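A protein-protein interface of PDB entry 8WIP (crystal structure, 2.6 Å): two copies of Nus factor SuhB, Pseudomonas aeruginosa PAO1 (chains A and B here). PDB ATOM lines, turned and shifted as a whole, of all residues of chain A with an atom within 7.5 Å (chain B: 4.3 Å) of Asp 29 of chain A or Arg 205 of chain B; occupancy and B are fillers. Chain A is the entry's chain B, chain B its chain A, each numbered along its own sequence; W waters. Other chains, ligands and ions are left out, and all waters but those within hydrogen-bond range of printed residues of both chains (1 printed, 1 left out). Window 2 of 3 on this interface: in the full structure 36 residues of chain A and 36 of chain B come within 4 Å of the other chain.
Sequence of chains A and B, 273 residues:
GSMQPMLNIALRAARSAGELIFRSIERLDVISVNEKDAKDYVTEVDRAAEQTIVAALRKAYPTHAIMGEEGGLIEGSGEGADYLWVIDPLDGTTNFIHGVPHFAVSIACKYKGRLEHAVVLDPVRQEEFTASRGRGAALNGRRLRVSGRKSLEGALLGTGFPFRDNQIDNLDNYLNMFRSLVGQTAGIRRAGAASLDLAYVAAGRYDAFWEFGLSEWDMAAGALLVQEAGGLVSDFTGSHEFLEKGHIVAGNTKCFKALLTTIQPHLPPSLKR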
ATOM      1  N   ARG A  23       6.609  -8.665  12.541  1.00  0.00           N
ATOM      2  CA  ARG A  23       7.954  -8.689  11.964  1.00  0.00           C
ATOM      3  C   ARG A  23       8.440  -7.265  11.709  1.00  0.00           C
ATOM      4  O   ARG A  23       9.631  -6.951  11.898  1.00  0.00           O
ATOM      5  CB  ARG A  23       7.942  -9.526  10.695  1.00  0.00           C
ATOM      6  CG  ARG A  23       7.317 -10.885  10.961  1.00  0.00           C
ATOM      7  CD  ARG A  23       7.508 -11.786   9.789  1.00  0.00           C
ATOM      8  NE  ARG A  23       7.544 -13.200  10.134  1.00  0.00           N
ATOM      9  CZ  ARG A  23       6.928 -14.155   9.445  1.00  0.00           C
ATOM     10  NH1 ARG A  23       6.223 -13.877   8.358  1.00  0.00           N
ATOM     11  NH2 ARG A  23       7.096 -15.428   9.801  1.00  0.00           N
ATOM     12  N   SER A  24       7.528  -6.399  11.249  1.00  0.00           N
ATOM     13  CA  SER A  24       7.871  -5.007  10.965  1.00  0.00           C
ATOM     14  C   SER A  24       8.363  -4.260  12.213  1.00  0.00           C
ATOM     15  O   SER A  24       9.339  -3.501  12.155  1.00  0.00           O
ATOM     16  CB  SER A  24       6.661  -4.302  10.381  1.00  0.00           C
ATOM     17  OG  SER A  24       7.126  -3.346   9.459  1.00  0.00           O
ATOM     18  N   ILE A  25       7.629  -4.379  13.327  1.00  0.00           N
ATOM     19  CA  ILE A  25       8.043  -3.677  14.544  1.00  0.00           C
ATOM     20  C   ILE A  25       9.396  -4.192  14.979  1.00  0.00           C
ATOM     21  O   ILE A  25      10.244  -3.439  15.481  1.00  0.00           O
ATOM     22  CB  ILE A  25       6.994  -3.767  15.678  1.00  0.00           C
ATOM     23  CG1 ILE A  25       7.408  -2.846  16.824  1.00  0.00           C
ATOM     24  CG2 ILE A  25       6.834  -5.181  16.258  1.00  0.00           C
ATOM     25  CD1 ILE A  25       6.249  -2.179  17.544  1.00  0.00           C
ATOM     26  N   GLU A  26       9.610  -5.494  14.813  1.00  0.00           N
ATOM     27  CA  GLU A  26      10.890  -6.055  15.212  1.00  0.00           C
ATOM     28  C   GLU A  26      12.030  -5.448  14.398  1.00  0.00           C
ATOM     29  O   GLU A  26      13.098  -5.139  14.945  1.00  0.00           O
ATOM     30  CB  GLU A  26      10.847  -7.576  15.100  1.00  0.00           C
ATOM     31  CG  GLU A  26       9.909  -8.229  16.095  1.00  0.00           C
ATOM     32  CD  GLU A  26      10.237  -9.680  16.242  1.00  0.00           C
ATOM     33  OE1 GLU A  26      10.234 -10.386  15.193  1.00  0.00           O
ATOM     34  OE2 GLU A  26      10.491 -10.121  17.388  1.00  0.00           O
ATOM     35  N   ARG A  27      11.819  -5.224  13.095  1.00  0.00           N
ATOM     36  CA  ARG A  27      12.926  -4.621  12.347  1.00  0.00           C
ATOM     37  C   ARG A  27      13.079  -3.150  12.712  1.00  0.00           C
ATOM     38  O   ARG A  27      14.202  -2.652  12.780  1.00  0.00           O
ATOM     39  CB  ARG A  27      12.771  -4.757  10.828  1.00  0.00           C
ATOM     40  CG  ARG A  27      12.254  -6.080  10.318  1.00  0.00           C
ATOM     41  CD  ARG A  27      12.422  -6.131   8.797  1.00  0.00           C
ATOM     42  NE  ARG A  27      11.469  -5.222   8.178  1.00  0.00           N
ATOM     43  CZ  ARG A  27      10.201  -5.533   7.930  1.00  0.00           C
ATOM     44  NH1 ARG A  27       9.694  -6.703   8.287  1.00  0.00           N
ATOM     45  NH2 ARG A  27       9.406  -4.624   7.358  1.00  0.00           N
ATOM     46  N   LEU A  28      11.981  -2.455  13.023  1.00  0.00           N
ATOM     47  CA  LEU A  28      12.105  -1.037  13.331  1.00  0.00           C
ATOM     48  C   LEU A  28      12.617  -0.718  14.742  1.00  0.00           C
ATOM     49  O   LEU A  28      13.172   0.378  14.926  1.00  0.00           O
ATOM     50  CB  LEU A  28      10.708  -0.418  13.184  1.00  0.00           C
ATOM     51  CG  LEU A  28      10.245   0.973  13.622  1.00  0.00           C
ATOM     52  CD1 LEU A  28       8.952   1.284  12.874  1.00  0.00           C
ATOM     53  CD2 LEU A  28       9.988   1.064  15.150  1.00  0.00           C
ATOM     54  N   ASP A  29      12.589  -1.670  15.710  1.00  0.00           N
ATOM     55  CA  ASP A  29      13.213  -1.334  17.001  1.00  0.00           C
ATOM     56  C   ASP A  29      14.729  -1.381  16.966  1.00  0.00           C
ATOM     57  O   ASP A  29      15.369  -0.780  17.841  1.00  0.00           O
ATOM     58  CB  ASP A  29      12.765  -2.234  18.176  1.00  0.00           C
ATOM     59  CG  ASP A  29      11.349  -1.937  18.664  1.00  0.00           C
ATOM     60  OD1 ASP A  29      10.938  -0.754  18.561  1.00  0.00           O
ATOM     61  OD2 ASP A  29      10.718  -2.813  19.312  1.00  0.00           O
ATOM     62  N   VAL A  30      15.310  -2.142  16.038  1.00  0.00           N
ATOM     63  CA  VAL A  30      16.755  -2.251  15.964  1.00  0.00           C
ATOM     64  C   VAL A  30      17.334  -1.332  14.893  1.00  0.00           C
ATOM     65  O   VAL A  30      18.553  -1.366  14.659  1.00  0.00           O
ATOM     66  CB  VAL A  30      17.189  -3.716  15.734  1.00  0.00           C
ATOM     67  CG1 VAL A  30      16.427  -4.631  16.681  1.00  0.00           C
ATOM     68  CG2 VAL A  30      17.026  -4.119  14.262  1.00  0.00           C
ATOM     69  N   ILE A  31      16.503  -0.497  14.245  1.00  0.00           N
ATOM     70  CA  ILE A  31      16.986   0.425  13.227  1.00  0.00           C
ATOM     71  C   ILE A  31      16.379   1.793  13.479  1.00  0.00           C
ATOM     72  O   ILE A  31      15.313   1.945  14.094  1.00  0.00           O
ATOM     73  CB  ILE A  31      16.776   0.025  11.741  1.00  0.00           C
ATOM     74  CG1 ILE A  31      15.353  -0.448  11.410  1.00  0.00           C
ATOM     75  CG2 ILE A  31      17.828  -1.013  11.349  1.00  0.00           C
ATOM     76  CD1 ILE A  31      14.330   0.683  11.152  1.00  0.00           C
ATOM     77  N   SER A  32      17.109   2.783  12.993  1.00  0.00           N
ATOM     78  CA  SER A  32      16.725   4.186  13.007  1.00  0.00           C
ATOM     79  C   SER A  32      15.517   4.528  12.139  1.00  0.00           C
ATOM     80  O   SER A  32      15.343   4.025  11.022  1.00  0.00           O
ATOM     81  CB  SER A  32      17.899   5.052  12.560  1.00  0.00           C
ATOM     82  OG  SER A  32      17.420   6.221  11.905  1.00  0.00           O
ATOM     83  N   VAL A  33      14.629   5.294  12.751  1.00  0.00           N
ATOM     84  CA  VAL A  33      13.356   5.745  12.220  1.00  0.00           C
ATOM     85  C   VAL A  33      13.663   7.232  12.064  1.00  0.00           C
ATOM     86  O   VAL A  33      13.631   7.994  13.046  1.00  0.00           O
ATOM     87  CB  VAL A  33      12.184   5.502  13.169  1.00  0.00           C
ATOM     88  CG1 VAL A  33      10.902   6.083  12.552  1.00  0.00           C
ATOM     89  CG2 VAL A  33      12.079   4.022  13.570  1.00  0.00           C
ATOM     90  N   TYR A  41       6.926   4.748   6.419  1.00  0.00           N
ATOM     91  CA  TYR A  41       7.034   3.379   6.909  1.00  0.00           C
ATOM     92  C   TYR A  41       5.714   2.877   7.483  1.00  0.00           C
ATOM     93  O   TYR A  41       5.332   1.722   7.256  1.00  0.00           O
ATOM     94  CB  TYR A  41       8.142   3.284   7.951  1.00  0.00           C
ATOM     95  CG  TYR A  41       8.539   1.861   8.167  1.00  0.00           C
ATOM     96  CD1 TYR A  41       8.761   1.011   7.086  1.00  0.00           C
ATOM     97  CD2 TYR A  41       8.615   1.339   9.445  1.00  0.00           C
ATOM     98  CE1 TYR A  41       9.094  -0.315   7.286  1.00  0.00           C
ATOM     99  CE2 TYR A  41       8.950   0.026   9.660  1.00  0.00           C
ATOM    100  CZ  TYR A  41       9.181  -0.803   8.583  1.00  0.00           C
ATOM    101  OH  TYR A  41       9.506  -2.127   8.829  1.00  0.00           O
ATOM    102  N   THR A  94       0.815   5.601  16.535  1.00  0.00           N
ATOM    103  CA  THR A  94       1.864   6.344  17.245  1.00  0.00           C
ATOM    104  C   THR A  94       2.729   5.416  18.111  1.00  0.00           C
ATOM    105  O   THR A  94       3.975   5.509  18.110  1.00  0.00           O
ATOM    106  CB  THR A  94       1.241   7.438  18.114  1.00  0.00           C
ATOM    107  OG1 THR A  94       0.602   8.412  17.287  1.00  0.00           O
ATOM    108  CG2 THR A  94       2.323   8.143  18.900  1.00  0.00           C
ATOM    109  N   ASN A  95       2.071   4.527  18.879  1.00  0.00           N
ATOM    110  CA  ASN A  95       2.755   3.447  19.583  1.00  0.00           C
ATOM    111  C   ASN A  95       3.645   2.646  18.650  1.00  0.00           C
ATOM    112  O   ASN A  95       4.834   2.445  18.921  1.00  0.00           O
ATOM    113  CB  ASN A  95       1.741   2.476  20.194  1.00  0.00           C
ATOM    114  CG  ASN A  95       1.084   2.994  21.439  1.00  0.00           C
ATOM    115  OD1 ASN A  95       1.383   4.079  21.932  1.00  0.00           O
ATOM    116  ND2 ASN A  95       0.157   2.219  21.947  1.00  0.00           N
ATOM    117  N   PHE A  96       3.073   2.171  17.546  1.00  0.00           N
ATOM    118  CA  PHE A  96       3.822   1.301  16.651  1.00  0.00           C
ATOM    119  C   PHE A  96       5.099   1.974  16.180  1.00  0.00           C
ATOM    120  O   PHE A  96       6.191   1.393  16.253  1.00  0.00           O
ATOM    121  CB  PHE A  96       2.971   0.873  15.459  1.00  0.00           C
ATOM    122  CG  PHE A  96       3.749   0.119  14.425  1.00  0.00           C
ATOM    123  CD1 PHE A  96       3.932  -1.246  14.547  1.00  0.00           C
ATOM    124  CD2 PHE A  96       4.309   0.768  13.336  1.00  0.00           C
ATOM    125  CE1 PHE A  96       4.649  -1.955  13.600  1.00  0.00           C
ATOM    126  CE2 PHE A  96       5.030   0.060  12.385  1.00  0.00           C
ATOM    127  CZ  PHE A  96       5.191  -1.307  12.518  1.00  0.00           C
ATOM    128  N   ILE A  97       4.975   3.201  15.670  1.00  0.00           N
ATOM    129  CA  ILE A  97       6.135   3.861  15.100  1.00  0.00           C
ATOM    130  C   ILE A  97       7.188   4.181  16.157  1.00  0.00           C
ATOM    131  O   ILE A  97       8.381   4.263  15.825  1.00  0.00           O
ATOM    132  CB  ILE A  97       5.667   5.111  14.334  1.00  0.00           C
ATOM    133  CG1 ILE A  97       6.706   5.523  13.315  1.00  0.00           C
ATOM    134  CG2 ILE A  97       5.387   6.249  15.269  1.00  0.00           C
ATOM    135  CD1 ILE A  97       7.260   4.378  12.501  1.00  0.00           C
ATOM    136  N   HIS A  98       6.796   4.308  17.430  1.00  0.00           N
ATOM    137  CA  HIS A  98       7.779   4.455  18.496  1.00  0.00           C
ATOM    138  C   HIS A  98       8.271   3.128  19.068  1.00  0.00           C
ATOM    139  O   HIS A  98       9.135   3.138  19.944  1.00  0.00           O
ATOM    140  CB  HIS A  98       7.219   5.300  19.624  1.00  0.00           C
ATOM    141  CG  HIS A  98       7.196   6.753  19.311  1.00  0.00           C
ATOM    142  ND1 HIS A  98       8.128   7.635  19.800  1.00  0.00           N
ATOM    143  CD2 HIS A  98       6.328   7.486  18.575  1.00  0.00           C
ATOM    144  CE1 HIS A  98       7.844   8.850  19.368  1.00  0.00           C
ATOM    145  NE2 HIS A  98       6.756   8.785  18.623  1.00  0.00           N
ATOM    146  N   GLY A  99       7.728   1.996  18.638  1.00  0.00           N
ATOM    147  CA  GLY A  99       8.108   0.724  19.214  1.00  0.00           C
ATOM    148  C   GLY A  99       7.372   0.327  20.478  1.00  0.00           C
ATOM    149  O   GLY A  99       7.728  -0.685  21.088  1.00  0.00           O
ATOM    150  N   VAL A 100       6.340   1.058  20.885  1.00  0.00           N
ATOM    151  CA  VAL A 100       5.561   0.666  22.057  1.00  0.00           C
ATOM    152  C   VAL A 100       4.747  -0.592  21.752  1.00  0.00           C
ATOM    153  O   VAL A 100       3.843  -0.557  20.913  1.00  0.00           O
ATOM    154  CB  VAL A 100       4.672   1.811  22.529  1.00  0.00           C
ATOM    155  CG1 VAL A 100       3.794   1.314  23.669  1.00  0.00           C
ATOM    156  CG2 VAL A 100       5.531   2.977  22.922  1.00  0.00           C
ATOM    157  N   PRO A 101       4.959  -1.698  22.436  1.00  0.00           N
ATOM    158  CA  PRO A 101       4.286  -2.944  22.010  1.00  0.00           C
ATOM    159  C   PRO A 101       2.832  -3.016  22.469  1.00  0.00           C
ATOM    160  O   PRO A 101       2.442  -3.830  23.307  1.00  0.00           O
ATOM    161  CB  PRO A 101       5.156  -4.024  22.671  1.00  0.00           C
ATOM    162  CG  PRO A 101       5.639  -3.357  23.928  1.00  0.00           C
ATOM    163  CD  PRO A 101       5.842  -1.902  23.597  1.00  0.00           C
ATOM    164  N   GLU B 127       9.773  -9.389  28.449  1.00  0.00           N
ATOM    165  CA  GLU B 127      10.759  -8.362  28.145  1.00  0.00           C
ATOM    166  C   GLU B 127      11.605  -8.111  29.387  1.00  0.00           C
ATOM    167  O   GLU B 127      11.080  -7.680  30.417  1.00  0.00           O
ATOM    168  CB  GLU B 127      10.098  -7.085  27.619  1.00  0.00           C
ATOM    169  CG  GLU B 127       9.458  -7.296  26.262  1.00  0.00           C
ATOM    170  CD  GLU B 127       9.218  -6.009  25.500  1.00  0.00           C
ATOM    171  OE1 GLU B 127       8.742  -5.032  26.133  1.00  0.00           O
ATOM    172  OE2 GLU B 127       9.483  -5.962  24.262  1.00  0.00           O
ATOM    173  N   PHE B 129      14.516  -5.965  30.811  1.00  0.00           N
ATOM    174  CA  PHE B 129      15.392  -4.802  30.764  1.00  0.00           C
ATOM    175  C   PHE B 129      16.412  -4.934  31.883  1.00  0.00           C
ATOM    176  O   PHE B 129      16.022  -5.066  33.044  1.00  0.00           O
ATOM    177  CB  PHE B 129      14.611  -3.501  30.937  1.00  0.00           C
ATOM    178  CG  PHE B 129      13.510  -3.322  29.935  1.00  0.00           C
ATOM    179  CD1 PHE B 129      12.242  -3.838  30.194  1.00  0.00           C
ATOM    180  CD2 PHE B 129      13.735  -2.649  28.734  1.00  0.00           C
ATOM    181  CE1 PHE B 129      11.222  -3.692  29.297  1.00  0.00           C
ATOM    182  CE2 PHE B 129      12.688  -2.502  27.818  1.00  0.00           C
ATOM    183  CZ  PHE B 129      11.425  -3.030  28.110  1.00  0.00           C
ATOM    184  N   LEU B 139      17.686  -4.878  26.372  1.00  0.00           N
ATOM    185  CA  LEU B 139      16.379  -5.542  26.384  1.00  0.00           C
ATOM    186  C   LEU B 139      16.583  -6.920  25.766  1.00  0.00           C
ATOM    187  O   LEU B 139      16.853  -7.027  24.563  1.00  0.00           O
ATOM    188  CB  LEU B 139      15.313  -4.738  25.632  1.00  0.00           C
ATOM    189  CG  LEU B 139      14.011  -5.482  25.267  1.00  0.00           C
ATOM    190  CD1 LEU B 139      13.332  -6.088  26.522  1.00  0.00           C
ATOM    191  CD2 LEU B 139      13.020  -4.579  24.529  1.00  0.00           C
ATOM    192  N   ARG B 142      20.060  -7.212  24.022  1.00  0.00           N
ATOM    193  CA  ARG B 142      20.376  -6.221  23.003  1.00  0.00           C
ATOM    194  C   ARG B 142      20.564  -4.827  23.602  1.00  0.00           C
ATOM    195  O   ARG B 142      19.693  -4.328  24.325  1.00  0.00           O
ATOM    196  CB  ARG B 142      19.199  -6.192  22.028  1.00  0.00           C
ATOM    197  CG  ARG B 142      18.898  -4.811  21.493  1.00  0.00           C
ATOM    198  CD  ARG B 142      18.243  -4.722  20.137  1.00  0.00           C
ATOM    199  NE  ARG B 142      16.825  -4.707  20.511  1.00  0.00           N
ATOM    200  CZ  ARG B 142      16.136  -3.596  20.747  1.00  0.00           C
ATOM    201  NH1 ARG B 142      16.681  -2.396  20.559  1.00  0.00           N
ATOM    202  NH2 ARG B 142      14.909  -3.688  21.270  1.00  0.00           N
ATOM    203  N   LEU B 156       6.562  11.211  21.931  1.00  0.00           N
ATOM    204  CA  LEU B 156       5.685  10.348  22.723  1.00  0.00           C
ATOM    205  C   LEU B 156       6.196  10.338  24.155  1.00  0.00           C
ATOM    206  O   LEU B 156       7.332   9.932  24.395  1.00  0.00           O
ATOM    207  CB  LEU B 156       5.615   8.934  22.144  1.00  0.00           C
ATOM    208  CG  LEU B 156       4.661   7.917  22.800  1.00  0.00           C
ATOM    209  CD1 LEU B 156       3.212   8.324  22.646  1.00  0.00           C
ATOM    210  CD2 LEU B 156       4.836   6.530  22.210  1.00  0.00           C
ATOM    211  N   TYR B 200      10.924   2.046  28.988  1.00  0.00           N
ATOM    212  CA  TYR B 200      10.604   2.441  27.627  1.00  0.00           C
ATOM    213  C   TYR B 200      11.380   3.674  27.223  1.00  0.00           C
ATOM    214  O   TYR B 200      11.759   3.814  26.052  1.00  0.00           O
ATOM    215  CB  TYR B 200       9.110   2.711  27.499  1.00  0.00           C
ATOM    216  CG  TYR B 200       8.267   1.472  27.421  1.00  0.00           C
ATOM    217  CD1 TYR B 200       8.781   0.237  27.803  1.00  0.00           C
ATOM    218  CD2 TYR B 200       6.966   1.532  26.951  1.00  0.00           C
ATOM    219  CE1 TYR B 200       8.019  -0.902  27.736  1.00  0.00           C
ATOM    220  CE2 TYR B 200       6.193   0.389  26.862  1.00  0.00           C
ATOM    221  CZ  TYR B 200       6.725  -0.816  27.261  1.00  0.00           C
ATOM    222  OH  TYR B 200       5.967  -1.949  27.190  1.00  0.00           O
ATOM    223  N   ALA B 203      14.751   2.239  26.283  1.00  0.00           N
ATOM    224  CA  ALA B 203      14.763   1.546  25.005  1.00  0.00           C
ATOM    225  C   ALA B 203      14.454   2.447  23.814  1.00  0.00           C
ATOM    226  O   ALA B 203      14.501   1.959  22.680  1.00  0.00           O
ATOM    227  CB  ALA B 203      13.765   0.384  25.044  1.00  0.00           C
ATOM    228  N   GLY B 204      14.133   3.727  24.024  1.00  0.00           N
ATOM    229  CA  GLY B 204      13.750   4.615  22.936  1.00  0.00           C
ATOM    230  C   GLY B 204      12.280   4.598  22.550  1.00  0.00           C
ATOM    231  O   GLY B 204      11.903   5.247  21.560  1.00  0.00           O
ATOM    232  N   ARG B 205      11.432   3.898  23.309  1.00  0.00           N
ATOM    233  CA  ARG B 205      10.018   3.813  22.980  1.00  0.00           C
ATOM    234  C   ARG B 205       9.246   5.046  23.422  1.00  0.00           C
ATOM    235  O   ARG B 205       8.217   5.371  22.819  1.00  0.00           O
ATOM    236  CB  ARG B 205       9.431   2.548  23.576  1.00  0.00           C
ATOM    237  CG  ARG B 205      10.226   1.317  23.246  1.00  0.00           C
ATOM    238  CD  ARG B 205       9.560   0.102  23.859  1.00  0.00           C
ATOM    239  NE  ARG B 205       9.944  -1.155  23.240  1.00  0.00           N
ATOM    240  CZ  ARG B 205       9.685  -2.345  23.755  1.00  0.00           C
ATOM    241  NH1 ARG B 205       9.044  -2.476  24.911  1.00  0.00           N
ATOM    242  NH2 ARG B 205      10.020  -3.432  23.068  1.00  0.00           N
ATOM    243  N   TYR B 206       9.656   5.680  24.516  1.00  0.00           N
ATOM    244  CA  TYR B 206       9.210   7.013  24.898  1.00  0.00           C
ATOM    245  C   TYR B 206      10.374   7.975  24.773  1.00  0.00           C
ATOM    246  O   TYR B 206      11.522   7.606  25.030  1.00  0.00           O
ATOM    247  CB  TYR B 206       8.761   7.090  26.348  1.00  0.00           C
ATOM    248  CG  TYR B 206       7.538   6.337  26.672  1.00  0.00           C
ATOM    249  CD1 TYR B 206       6.633   5.960  25.687  1.00  0.00           C
ATOM    250  CD2 TYR B 206       7.278   5.993  27.982  1.00  0.00           C
ATOM    251  CE1 TYR B 206       5.501   5.238  26.027  1.00  0.00           C
ATOM    252  CE2 TYR B 206       6.173   5.303  28.318  1.00  0.00           C
ATOM    253  CZ  TYR B 206       5.290   4.922  27.357  1.00  0.00           C
ATOM    254  OH  TYR B 206       4.188   4.205  27.764  1.00  0.00           O
HETATM  255  O   HOH W   1      10.345   7.431  21.569  1.00  0.00           O
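No position is printed for both chains.
Hydrophobic or aromatic side chains of chain B that line the printed part of chain A: Leu 156, Tyr 200 and Tyr 206.
Printed residues of chain A that touch a printed residue of chain B: Asp 29, Val 30, Thr 94, His 98, Gly 99, Val 100 and Pro 101.
Hydrophobic or aromatic side chains of chain A within 4 Å of the printed part of chain B: Val 30, His 98, Val 100 and Pro 101.
Water W1 lies within hydrogen-bond range of the backbone carbonyl oxygen of Gly 204 of chain B, a ring nitrogen (ND1) of His 98 of chain A, the backbone carbonyl oxygen of Arg 205 of chain B and the backbone NH of Tyr 206 of chain B.
Arg 142 of chain B touches Val 30 of chain A.
Thr 94 of chain A touches Leu 156 of chain B.
CE1 of His 98 of chain A touches CB of Leu 156 of chain B, at 3.6 Å.
His 98 of chain A touches Gly 204 of chain B.
O of His 98 of chain A touches CA of Arg 205 of chain B, at 3.2 Å.
CG2 of Val 100 of chain A touches CD2 of Leu 156 of chain B, at 3.7 Å.
Val 100 of chain A touches Arg 205 of chain B.
CG2 of Val 100 of chain A touches CE1 of Tyr 206 of chain B, 3.8 Å away.
Pro 101 of chain A touches Tyr 200 of chain B.
Pro 101 of chain A touches Arg 205 of chain B.
O of Asp 29 of chain A is in hydrogen-bond range of NH1 of Arg 142 of chain B, 3.4 Å away.
The guanidinium group (NH2) of Arg 205 of chain B is in salt-bridge range of the side-chain carboxylate (OD2) of Asp 29 of chain A (3.9 Å).
The backbone carbonyl oxygen (O) of Gly 99 of chain A lies within hydrogen-bond range of the guanidinium group (NE) of Arg 205 of chain B (3.1 Å).
NH1 of Arg 205 of chain B lies within salt-bridge range of OE1 of Glu 127 of chain B.
O of Tyr 200 of chain B sits at hydrogen-bond distance from N of Arg 205 of chain B, 2.8 Å away.
O of Tyr 200 of chain B sits at hydrogen-bond distance from N of Tyr 206 of chain B (3.2 Å).
The backbone carbonyl oxygen of Asn 95 of chain A sits at hydrogen-bond distance from the backbone NH of Val 100 of chain A, 2.8 Å away.
Of chain B, only Arg 142 and Arg 205 come within 4 Å of Asp 29 of chain A.
Arg 205 of chain B touches five residues of chain A.
Of the printed residues of chain B, Pro 101 of chain A touches Tyr 200 and Arg 205.
Of the printed residues of chain A, Arg 142 of chain B touches Asp 29 (3.4 Å) and Val 30 (3.9 Å).
Phe 96 of chain A touches none of the printed residues of chain B.
The nearest residue of chain A that does not touch Arg 205 of chain B is Asn 95 of chain A (5.9 Å).
The nearest printed residue of chain A that does not touch Tyr 206 of chain B is His 98 of chain A (5.2 Å).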
